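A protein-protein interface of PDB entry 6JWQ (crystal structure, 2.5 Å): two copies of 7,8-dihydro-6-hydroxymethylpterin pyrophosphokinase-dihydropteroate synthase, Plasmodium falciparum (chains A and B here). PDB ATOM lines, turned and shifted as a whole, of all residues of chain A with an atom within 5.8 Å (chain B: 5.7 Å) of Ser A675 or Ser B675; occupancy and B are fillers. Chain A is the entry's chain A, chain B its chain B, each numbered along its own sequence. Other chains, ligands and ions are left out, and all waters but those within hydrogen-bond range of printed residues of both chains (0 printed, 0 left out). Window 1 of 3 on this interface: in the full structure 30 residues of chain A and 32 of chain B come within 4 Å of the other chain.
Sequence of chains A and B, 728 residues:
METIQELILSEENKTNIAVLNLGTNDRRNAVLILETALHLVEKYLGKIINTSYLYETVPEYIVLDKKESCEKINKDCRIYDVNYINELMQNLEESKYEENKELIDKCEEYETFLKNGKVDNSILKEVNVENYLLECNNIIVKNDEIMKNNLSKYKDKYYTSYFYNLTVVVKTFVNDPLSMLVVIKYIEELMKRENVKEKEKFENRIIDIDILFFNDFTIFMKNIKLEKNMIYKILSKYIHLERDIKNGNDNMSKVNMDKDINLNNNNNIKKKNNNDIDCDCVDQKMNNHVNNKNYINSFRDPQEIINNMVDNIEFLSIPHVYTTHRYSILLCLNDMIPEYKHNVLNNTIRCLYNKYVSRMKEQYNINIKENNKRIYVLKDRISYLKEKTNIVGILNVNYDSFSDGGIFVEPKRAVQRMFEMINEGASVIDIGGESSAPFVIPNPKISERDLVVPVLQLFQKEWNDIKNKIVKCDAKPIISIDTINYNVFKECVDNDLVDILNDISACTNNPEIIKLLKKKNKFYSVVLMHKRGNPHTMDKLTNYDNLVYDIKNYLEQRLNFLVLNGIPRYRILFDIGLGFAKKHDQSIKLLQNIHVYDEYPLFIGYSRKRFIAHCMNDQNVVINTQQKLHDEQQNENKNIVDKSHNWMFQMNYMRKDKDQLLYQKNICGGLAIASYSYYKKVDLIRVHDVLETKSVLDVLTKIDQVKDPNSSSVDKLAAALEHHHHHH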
ATOM      1  N   GLY A 670     -26.083  -5.985  38.231  1.00  0.00           N
ATOM      2  CA  GLY A 670     -26.689  -6.999  37.383  1.00  0.00           C
ATOM      3  C   GLY A 670     -27.246  -6.411  36.096  1.00  0.00           C
ATOM      4  O   GLY A 670     -27.021  -6.957  35.001  1.00  0.00           O
ATOM      5  N   LEU A 671     -27.949  -5.278  36.223  1.00  0.00           N
ATOM      6  CA  LEU A 671     -28.481  -4.575  35.051  1.00  0.00           C
ATOM      7  C   LEU A 671     -27.394  -4.102  34.067  1.00  0.00           C
ATOM      8  O   LEU A 671     -27.575  -4.233  32.871  1.00  0.00           O
ATOM      9  CB  LEU A 671     -29.462  -3.484  35.466  1.00  0.00           C
ATOM     10  CG  LEU A 671     -30.664  -4.076  36.226  1.00  0.00           C
ATOM     11  CD1 LEU A 671     -31.569  -2.986  36.790  1.00  0.00           C
ATOM     12  CD2 LEU A 671     -31.464  -5.071  35.380  1.00  0.00           C
ATOM     13  N   ALA A 672     -26.249  -3.632  34.570  1.00  0.00           N
ATOM     14  CA  ALA A 672     -25.058  -3.428  33.732  1.00  0.00           C
ATOM     15  C   ALA A 672     -24.656  -4.664  32.927  1.00  0.00           C
ATOM     16  O   ALA A 672     -24.420  -4.558  31.713  1.00  0.00           O
ATOM     17  CB  ALA A 672     -23.882  -2.940  34.548  1.00  0.00           C
ATOM     18  N   ILE A 673     -24.593  -5.830  33.581  1.00  0.00           N
ATOM     19  CA  ILE A 673     -24.277  -7.098  32.884  1.00  0.00           C
ATOM     20  C   ILE A 673     -25.413  -7.495  31.905  1.00  0.00           C
ATOM     21  O   ILE A 673     -25.126  -8.055  30.840  1.00  0.00           O
ATOM     22  CB  ILE A 673     -23.827  -8.245  33.845  1.00  0.00           C
ATOM     23  CG1 ILE A 673     -22.816  -7.702  34.876  1.00  0.00           C
ATOM     24  CG2 ILE A 673     -23.188  -9.394  33.075  1.00  0.00           C
ATOM     25  CD1 ILE A 673     -22.247  -8.700  35.874  1.00  0.00           C
ATOM     26  N   ALA A 674     -26.673  -7.179  32.221  1.00  0.00           N
ATOM     27  CA  ALA A 674     -27.748  -7.383  31.237  1.00  0.00           C
ATOM     28  C   ALA A 674     -27.483  -6.586  29.939  1.00  0.00           C
ATOM     29  O   ALA A 674     -27.661  -7.106  28.827  1.00  0.00           O
ATOM     30  CB  ALA A 674     -29.117  -7.033  31.818  1.00  0.00           C
ATOM     31  N   SER A 675     -27.032  -5.339  30.095  1.00  0.00           N
ATOM     32  CA  SER A 675     -26.695  -4.452  28.972  1.00  0.00           C
ATOM     33  C   SER A 675     -25.554  -4.984  28.144  1.00  0.00           C
ATOM     34  O   SER A 675     -25.629  -4.994  26.914  1.00  0.00           O
ATOM     35  CB  SER A 675     -26.335  -3.055  29.469  1.00  0.00           C
ATOM     36  OG  SER A 675     -27.430  -2.483  30.165  1.00  0.00           O
ATOM     37  N   TYR A 676     -24.511  -5.446  28.827  1.00  0.00           N
ATOM     38  CA  TYR A 676     -23.338  -6.004  28.183  1.00  0.00           C
ATOM     39  C   TYR A 676     -23.717  -7.278  27.414  1.00  0.00           C
ATOM     40  O   TYR A 676     -23.305  -7.464  26.260  1.00  0.00           O
ATOM     41  CB  TYR A 676     -22.266  -6.265  29.255  1.00  0.00           C
ATOM     42  CG  TYR A 676     -20.982  -6.860  28.736  1.00  0.00           C
ATOM     43  CD1 TYR A 676     -20.076  -6.083  27.990  1.00  0.00           C
ATOM     44  CD2 TYR A 676     -20.659  -8.201  29.000  1.00  0.00           C
ATOM     45  CE1 TYR A 676     -18.887  -6.634  27.509  1.00  0.00           C
ATOM     46  CE2 TYR A 676     -19.468  -8.760  28.532  1.00  0.00           C
ATOM     47  CZ  TYR A 676     -18.585  -7.973  27.794  1.00  0.00           C
ATOM     48  OH  TYR A 676     -17.412  -8.512  27.325  1.00  0.00           O
ATOM     49  N   SER A 677     -24.528  -8.118  28.064  1.00  0.00           N
ATOM     50  CA  SER A 677     -25.038  -9.374  27.514  1.00  0.00           C
ATOM     51  C   SER A 677     -25.842  -9.131  26.268  1.00  0.00           C
ATOM     52  O   SER A 677     -25.715  -9.886  25.308  1.00  0.00           O
ATOM     53  CB  SER A 677     -25.926 -10.109  28.532  1.00  0.00           C
ATOM     54  OG  SER A 677     -25.173 -10.491  29.668  1.00  0.00           O
ATOM     55  N   TYR A 678     -26.682  -8.091  26.304  1.00  0.00           N
ATOM     56  CA  TYR A 678     -27.453  -7.665  25.146  1.00  0.00           C
ATOM     57  C   TYR A 678     -26.562  -7.349  23.918  1.00  0.00           C
ATOM     58  O   TYR A 678     -26.802  -7.856  22.810  1.00  0.00           O
ATOM     59  CB  TYR A 678     -28.338  -6.453  25.489  1.00  0.00           C
ATOM     60  CG  TYR A 678     -29.010  -5.896  24.256  1.00  0.00           C
ATOM     61  CD1 TYR A 678     -30.199  -6.467  23.768  1.00  0.00           C
ATOM     62  CD2 TYR A 678     -28.428  -4.842  23.534  1.00  0.00           C
ATOM     63  CE1 TYR A 678     -30.801  -5.987  22.619  1.00  0.00           C
ATOM     64  CE2 TYR A 678     -29.025  -4.355  22.390  1.00  0.00           C
ATOM     65  CZ  TYR A 678     -30.202  -4.936  21.937  1.00  0.00           C
ATOM     66  OH  TYR A 678     -30.784  -4.464  20.803  1.00  0.00           O
ATOM     67  N   TYR A 679     -25.559  -6.503  24.126  1.00  0.00           N
ATOM     68  CA  TYR A 679     -24.621  -6.132  23.078  1.00  0.00           C
ATOM     69  C   TYR A 679     -23.726  -7.271  22.655  1.00  0.00           C
ATOM     70  O   TYR A 679     -23.315  -7.325  21.501  1.00  0.00           O
ATOM     71  CB  TYR A 679     -23.794  -4.910  23.490  1.00  0.00           C
ATOM     72  CG  TYR A 679     -24.641  -3.668  23.540  1.00  0.00           C
ATOM     73  CD1 TYR A 679     -25.381  -3.262  22.412  1.00  0.00           C
ATOM     74  CD2 TYR A 679     -24.721  -2.889  24.706  1.00  0.00           C
ATOM     75  CE1 TYR A 679     -26.176  -2.136  22.449  1.00  0.00           C
ATOM     76  CE2 TYR A 679     -25.529  -1.757  24.750  1.00  0.00           C
ATOM     77  CZ  TYR A 679     -26.247  -1.393  23.617  1.00  0.00           C
ATOM     78  OH  TYR A 679     -27.058  -0.289  23.635  1.00  0.00           O
ATOM     79  N   LYS A 680     -23.427  -8.194  23.567  1.00  0.00           N
ATOM     80  CA  LYS A 680     -22.606  -9.353  23.205  1.00  0.00           C
ATOM     81  C   LYS A 680     -23.467 -10.469  22.654  1.00  0.00           C
ATOM     82  O   LYS A 680     -22.960 -11.541  22.311  1.00  0.00           O
ATOM     83  CB  LYS A 680     -21.716  -9.806  24.353  1.00  0.00           C
ATOM     84  CG  LYS A 680     -20.629  -8.819  24.734  1.00  0.00           C
ATOM     85  CD  LYS A 680     -19.719  -8.507  23.566  1.00  0.00           C
ATOM     86  CE  LYS A 680     -18.496  -7.693  23.965  1.00  0.00           C
ATOM     87  NZ  LYS A 680     -17.296  -8.071  23.152  1.00  0.00           N
ATOM     88  N   VAL A 696     -34.520  -2.996  31.010  1.00  0.00           N
ATOM     89  CA  VAL A 696     -33.264  -2.718  30.334  1.00  0.00           C
ATOM     90  C   VAL A 696     -33.344  -3.238  28.889  1.00  0.00           C
ATOM     91  O   VAL A 696     -33.116  -2.470  27.937  1.00  0.00           O
ATOM     92  CB  VAL A 696     -32.012  -3.206  31.120  1.00  0.00           C
ATOM     93  CG1 VAL A 696     -30.745  -3.095  30.276  1.00  0.00           C
ATOM     94  CG2 VAL A 696     -31.831  -2.405  32.402  1.00  0.00           C
ATOM     95  N   LEU A 697     -33.733  -4.499  28.704  1.00  0.00           N
ATOM     96  CA  LEU A 697     -33.660  -5.096  27.351  1.00  0.00           C
ATOM     97  C   LEU A 697     -34.607  -4.444  26.337  1.00  0.00           C
ATOM     98  O   LEU A 697     -34.274  -4.358  25.150  1.00  0.00           O
ATOM     99  CB  LEU A 697     -33.786  -6.630  27.370  1.00  0.00           C
ATOM    100  CG  LEU A 697     -32.735  -7.446  28.159  1.00  0.00           C
ATOM    101  CD1 LEU A 697     -33.013  -8.932  28.067  1.00  0.00           C
ATOM    102  CD2 LEU A 697     -31.299  -7.213  27.726  1.00  0.00           C
ATOM    103  N   LEU A 700     -32.889  -0.959  25.305  1.00  0.00           N
ATOM    104  CA  LEU A 700     -31.776  -1.168  24.367  1.00  0.00           C
ATOM    105  C   LEU A 700     -32.234  -1.636  22.982  1.00  0.00           C
ATOM    106  O   LEU A 700     -31.659  -1.222  21.963  1.00  0.00           O
ATOM    107  CB  LEU A 700     -30.716  -2.108  24.945  1.00  0.00           C
ATOM    108  CG  LEU A 700     -30.114  -1.704  26.292  1.00  0.00           C
ATOM    109  CD1 LEU A 700     -29.163  -2.791  26.769  1.00  0.00           C
ATOM    110  CD2 LEU A 700     -29.416  -0.359  26.216  1.00  0.00           C
ATOM    111  N   GLY B 670     -34.061   3.756  32.339  1.00  0.00           N
ATOM    112  CA  GLY B 670     -33.023   4.750  32.430  1.00  0.00           C
ATOM    113  C   GLY B 670     -31.640   4.168  32.544  1.00  0.00           C
ATOM    114  O   GLY B 670     -30.701   4.674  31.917  1.00  0.00           O
ATOM    115  N   LEU B 671     -31.504   3.096  33.332  1.00  0.00           N
ATOM    116  CA  LEU B 671     -30.207   2.440  33.548  1.00  0.00           C
ATOM    117  C   LEU B 671     -29.677   1.821  32.245  1.00  0.00           C
ATOM    118  O   LEU B 671     -28.462   1.789  32.000  1.00  0.00           O
ATOM    119  CB  LEU B 671     -30.281   1.434  34.701  1.00  0.00           C
ATOM    120  CG  LEU B 671     -30.484   2.037  36.107  1.00  0.00           C
ATOM    121  CD1 LEU B 671     -30.637   0.942  37.151  1.00  0.00           C
ATOM    122  CD2 LEU B 671     -29.358   2.986  36.512  1.00  0.00           C
ATOM    123  N   ALA B 672     -30.601   1.396  31.389  1.00  0.00           N
ATOM    124  CA  ALA B 672     -30.253   0.997  30.035  1.00  0.00           C
ATOM    125  C   ALA B 672     -29.642   2.179  29.232  1.00  0.00           C
ATOM    126  O   ALA B 672     -28.665   1.992  28.490  1.00  0.00           O
ATOM    127  CB  ALA B 672     -31.470   0.413  29.321  1.00  0.00           C
ATOM    128  N   ILE B 673     -30.202   3.382  29.391  1.00  0.00           N
ATOM    129  CA  ILE B 673     -29.664   4.554  28.712  1.00  0.00           C
ATOM    130  C   ILE B 673     -28.310   4.956  29.299  1.00  0.00           C
ATOM    131  O   ILE B 673     -27.440   5.429  28.565  1.00  0.00           O
ATOM    132  CB  ILE B 673     -30.659   5.737  28.642  1.00  0.00           C
ATOM    133  CG1 ILE B 673     -31.948   5.276  27.967  1.00  0.00           C
ATOM    134  CG2 ILE B 673     -30.066   6.887  27.818  1.00  0.00           C
ATOM    135  CD1 ILE B 673     -33.123   6.213  28.142  1.00  0.00           C
ATOM    136  N   ALA B 674     -28.120   4.758  30.600  1.00  0.00           N
ATOM    137  CA  ALA B 674     -26.785   4.946  31.199  1.00  0.00           C
ATOM    138  C   ALA B 674     -25.754   4.035  30.541  1.00  0.00           C
ATOM    139  O   ALA B 674     -24.638   4.470  30.300  1.00  0.00           O
ATOM    140  CB  ALA B 674     -26.806   4.712  32.699  1.00  0.00           C
ATOM    141  N   SER B 675     -26.143   2.789  30.242  1.00  0.00           N
ATOM    142  CA  SER B 675     -25.242   1.806  29.618  1.00  0.00           C
ATOM    143  C   SER B 675     -24.881   2.223  28.209  1.00  0.00           C
ATOM    144  O   SER B 675     -23.699   2.160  27.809  1.00  0.00           O
ATOM    145  CB  SER B 675     -25.865   0.410  29.562  1.00  0.00           C
ATOM    146  OG  SER B 675     -26.174  -0.049  30.858  1.00  0.00           O
ATOM    147  N   TYR B 676     -25.917   2.628  27.468  1.00  0.00           N
ATOM    148  CA  TYR B 676     -25.788   3.120  26.109  1.00  0.00           C
ATOM    149  C   TYR B 676     -24.888   4.345  26.107  1.00  0.00           C
ATOM    150  O   TYR B 676     -23.950   4.398  25.319  1.00  0.00           O
ATOM    151  CB  TYR B 676     -27.168   3.424  25.520  1.00  0.00           C
ATOM    152  CG  TYR B 676     -27.142   3.912  24.089  1.00  0.00           C
ATOM    153  CD1 TYR B 676     -26.840   3.024  23.032  1.00  0.00           C
ATOM    154  CD2 TYR B 676     -27.417   5.267  23.779  1.00  0.00           C
ATOM    155  CE1 TYR B 676     -26.818   3.464  21.717  1.00  0.00           C
ATOM    156  CE2 TYR B 676     -27.387   5.722  22.462  1.00  0.00           C
ATOM    157  CZ  TYR B 676     -27.090   4.818  21.442  1.00  0.00           C
ATOM    158  OH  TYR B 676     -27.068   5.225  20.139  1.00  0.00           O
ATOM    159  N   SER B 677     -25.132   5.274  27.038  1.00  0.00           N
ATOM    160  CA  SER B 677     -24.341   6.510  27.204  1.00  0.00           C
ATOM    161  C   SER B 677     -22.883   6.229  27.494  1.00  0.00           C
ATOM    162  O   SER B 677     -21.989   6.873  26.925  1.00  0.00           O
ATOM    163  CB  SER B 677     -24.919   7.380  28.325  1.00  0.00           C
ATOM    164  OG  SER B 677     -26.228   7.820  28.007  1.00  0.00           O
ATOM    165  N   TYR B 678     -22.658   5.267  28.385  1.00  0.00           N
ATOM    166  CA  TYR B 678     -21.343   4.748  28.670  1.00  0.00           C
ATOM    167  C   TYR B 678     -20.620   4.308  27.400  1.00  0.00           C
ATOM    168  O   TYR B 678     -19.462   4.714  27.178  1.00  0.00           O
ATOM    169  CB  TYR B 678     -21.388   3.584  29.694  1.00  0.00           C
ATOM    170  CG  TYR B 678     -20.012   2.983  29.898  1.00  0.00           C
ATOM    171  CD1 TYR B 678     -19.096   3.579  30.763  1.00  0.00           C
ATOM    172  CD2 TYR B 678     -19.597   1.850  29.164  1.00  0.00           C
ATOM    173  CE1 TYR B 678     -17.822   3.053  30.935  1.00  0.00           C
ATOM    174  CE2 TYR B 678     -18.326   1.326  29.325  1.00  0.00           C
ATOM    175  CZ  TYR B 678     -17.446   1.938  30.208  1.00  0.00           C
ATOM    176  OH  TYR B 678     -16.181   1.437  30.369  1.00  0.00           O
ATOM    177  N   TYR B 679     -21.274   3.474  26.582  1.00  0.00           N
ATOM    178  CA  TYR B 679     -20.599   2.935  25.383  1.00  0.00           C
ATOM    179  C   TYR B 679     -20.435   3.970  24.309  1.00  0.00           C
ATOM    180  O   TYR B 679     -19.536   3.851  23.482  1.00  0.00           O
ATOM    181  CB  TYR B 679     -21.279   1.685  24.819  1.00  0.00           C
ATOM    182  CG  TYR B 679     -21.108   0.494  25.725  1.00  0.00           C
ATOM    183  CD1 TYR B 679     -19.832  -0.021  25.994  1.00  0.00           C
ATOM    184  CD2 TYR B 679     -22.205  -0.105  26.334  1.00  0.00           C
ATOM    185  CE1 TYR B 679     -19.661  -1.087  26.837  1.00  0.00           C
ATOM    186  CE2 TYR B 679     -22.038  -1.180  27.185  1.00  0.00           C
ATOM    187  CZ  TYR B 679     -20.763  -1.662  27.428  1.00  0.00           C
ATOM    188  OH  TYR B 679     -20.571  -2.745  28.264  1.00  0.00           O
ATOM    189  N   LYS B 680     -21.295   4.988  24.334  1.00  0.00           N
ATOM    190  CA  LYS B 680     -21.221   6.078  23.380  1.00  0.00           C
ATOM    191  C   LYS B 680     -20.320   7.197  23.874  1.00  0.00           C
ATOM    192  O   LYS B 680     -20.080   8.168  23.157  1.00  0.00           O
ATOM    193  CB  LYS B 680     -22.614   6.573  23.041  1.00  0.00           C
ATOM    194  CG  LYS B 680     -23.405   5.575  22.193  1.00  0.00           C
ATOM    195  CD  LYS B 680     -22.686   5.284  20.898  1.00  0.00           C
ATOM    196  CE  LYS B 680     -23.522   4.526  19.891  1.00  0.00           C
ATOM    197  NZ  LYS B 680     -22.910   4.756  18.529  1.00  0.00           N
ATOM    198  N   VAL B 696     -24.221   0.683  37.904  1.00  0.00           N
ATOM    199  CA  VAL B 696     -24.126   0.358  36.477  1.00  0.00           C
ATOM    200  C   VAL B 696     -22.784   0.796  35.883  1.00  0.00           C
ATOM    201  O   VAL B 696     -22.116   0.006  35.219  1.00  0.00           O
ATOM    202  CB  VAL B 696     -25.310   0.929  35.674  1.00  0.00           C
ATOM    203  CG1 VAL B 696     -25.021   0.963  34.181  1.00  0.00           C
ATOM    204  CG2 VAL B 696     -26.561   0.110  35.941  1.00  0.00           C
ATOM    205  N   LEU B 697     -22.378   2.033  36.139  1.00  0.00           N
ATOM    206  CA  LEU B 697     -21.164   2.538  35.503  1.00  0.00           C
ATOM    207  C   LEU B 697     -19.907   1.866  36.041  1.00  0.00           C
ATOM    208  O   LEU B 697     -18.952   1.656  35.298  1.00  0.00           O
ATOM    209  CB  LEU B 697     -21.085   4.070  35.567  1.00  0.00           C
ATOM    210  CG  LEU B 697     -22.155   4.898  34.814  1.00  0.00           C
ATOM    211  CD1 LEU B 697     -21.823   6.386  34.888  1.00  0.00           C
ATOM    212  CD2 LEU B 697     -22.357   4.495  33.358  1.00  0.00           C
ATOM    213  N   LEU B 700     -19.601  -1.663  34.242  1.00  0.00           N
ATOM    214  CA  LEU B 700     -19.193  -1.526  32.861  1.00  0.00           C
ATOM    215  C   LEU B 700     -17.752  -1.077  32.763  1.00  0.00           C
ATOM    216  O   LEU B 700     -17.031  -1.548  31.888  1.00  0.00           O
ATOM    217  CB  LEU B 700     -20.131  -0.638  32.045  1.00  0.00           C
ATOM    218  CG  LEU B 700     -21.600  -1.100  32.024  1.00  0.00           C
ATOM    219  CD1 LEU B 700     -22.487  -0.008  31.443  1.00  0.00           C
ATOM    220  CD2 LEU B 700     -21.812  -2.438  31.325  1.00  0.00           C
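The side-chain hydroxyl of Ser A675 sits at hydrogen-bond distance from the side-chain hydroxyl of Ser B675 (2.8 Å).
The side-chain hydroxyl (OH) of Tyr B678 is in hydrogen-bond range of the backbone carbonyl oxygen (O) of Leu B700. The backbone carbonyl oxygen (O) of Leu A671 is in hydrogen-bond range of the side-chain hydroxyl (OG) of Ser A675, at 3.2 Å. O of Leu B671 is in hydrogen-bond range of OG of Ser B675 (3.1 Å).
Among the printed residues, merely in contact across the chains: Leu A700 with Ala B672 (3.4 Å), Tyr A679 with Tyr B676 (3.4 Å), Ala A672 with Leu B700 (3.4 Å), Tyr A676 with Tyr B679 (3.4 Å), Ala A672 with Val B696 (3.5 Å) and Val A696 with Ala B672 (3.6 Å).
Printed residues of chain B within 4 Å of Ala A672: Val B696 and Leu B700. Of chain B, only Ser B675 comes within 4 Å of Ser A675. Of the printed residues of chain B, Tyr A679 touches Tyr B676. Of chain A, only Ser A675 comes within 4 Å of Ser B675. Of the printed residues of chain A, Tyr B679 touches Tyr A676. Of the printed residues of chain A, Val B696 touches Ala A672 (3.5 Å). Of the printed residues of chain A, Leu B700 touches Ala A672 (3.4 Å). The nearest residue of chain A that does not touch Ser B675 is Ala A672 (4.6 Å). The nearest printed residue of chain B that does not touch Ala A672 is Ser B675 (4.6 Å).
Hydrophobic or aromatic side chains of chain A within 4 Å of the printed part of chain B: Ala A672, Tyr A676, Tyr A679, Val A696 and Leu A700. Hydrophobic or aromatic side chains of chain B within 4 Å of the printed part of chain A: Ala B672, Tyr B676, Tyr B679, Val B696 and Leu B700. Along chain B the printed residues that touch a printed residue of chain A span positions 672 to 700. Among the printed residues, no Asp or Glu carboxylate lies within 4 Å of a Lys or Arg side-chain nitrogen of the other chain.
Ala A672 touches Val B696, and with the chains exchanged Val A696 touches Ala B672. Ala A672 touches Leu B700, and with the chains exchanged Leu A700 touches Ala B672. Ser B675 touches its own counterpart, Ser A675. Tyr A676 touches Tyr B679, and with the chains exchanged Tyr A679 touches Tyr B676. 14 positions are printed for both chains. Of the 7 pairs that touch across the chains among the printed residues, 7 have their exchanged pair printed and touching as well.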
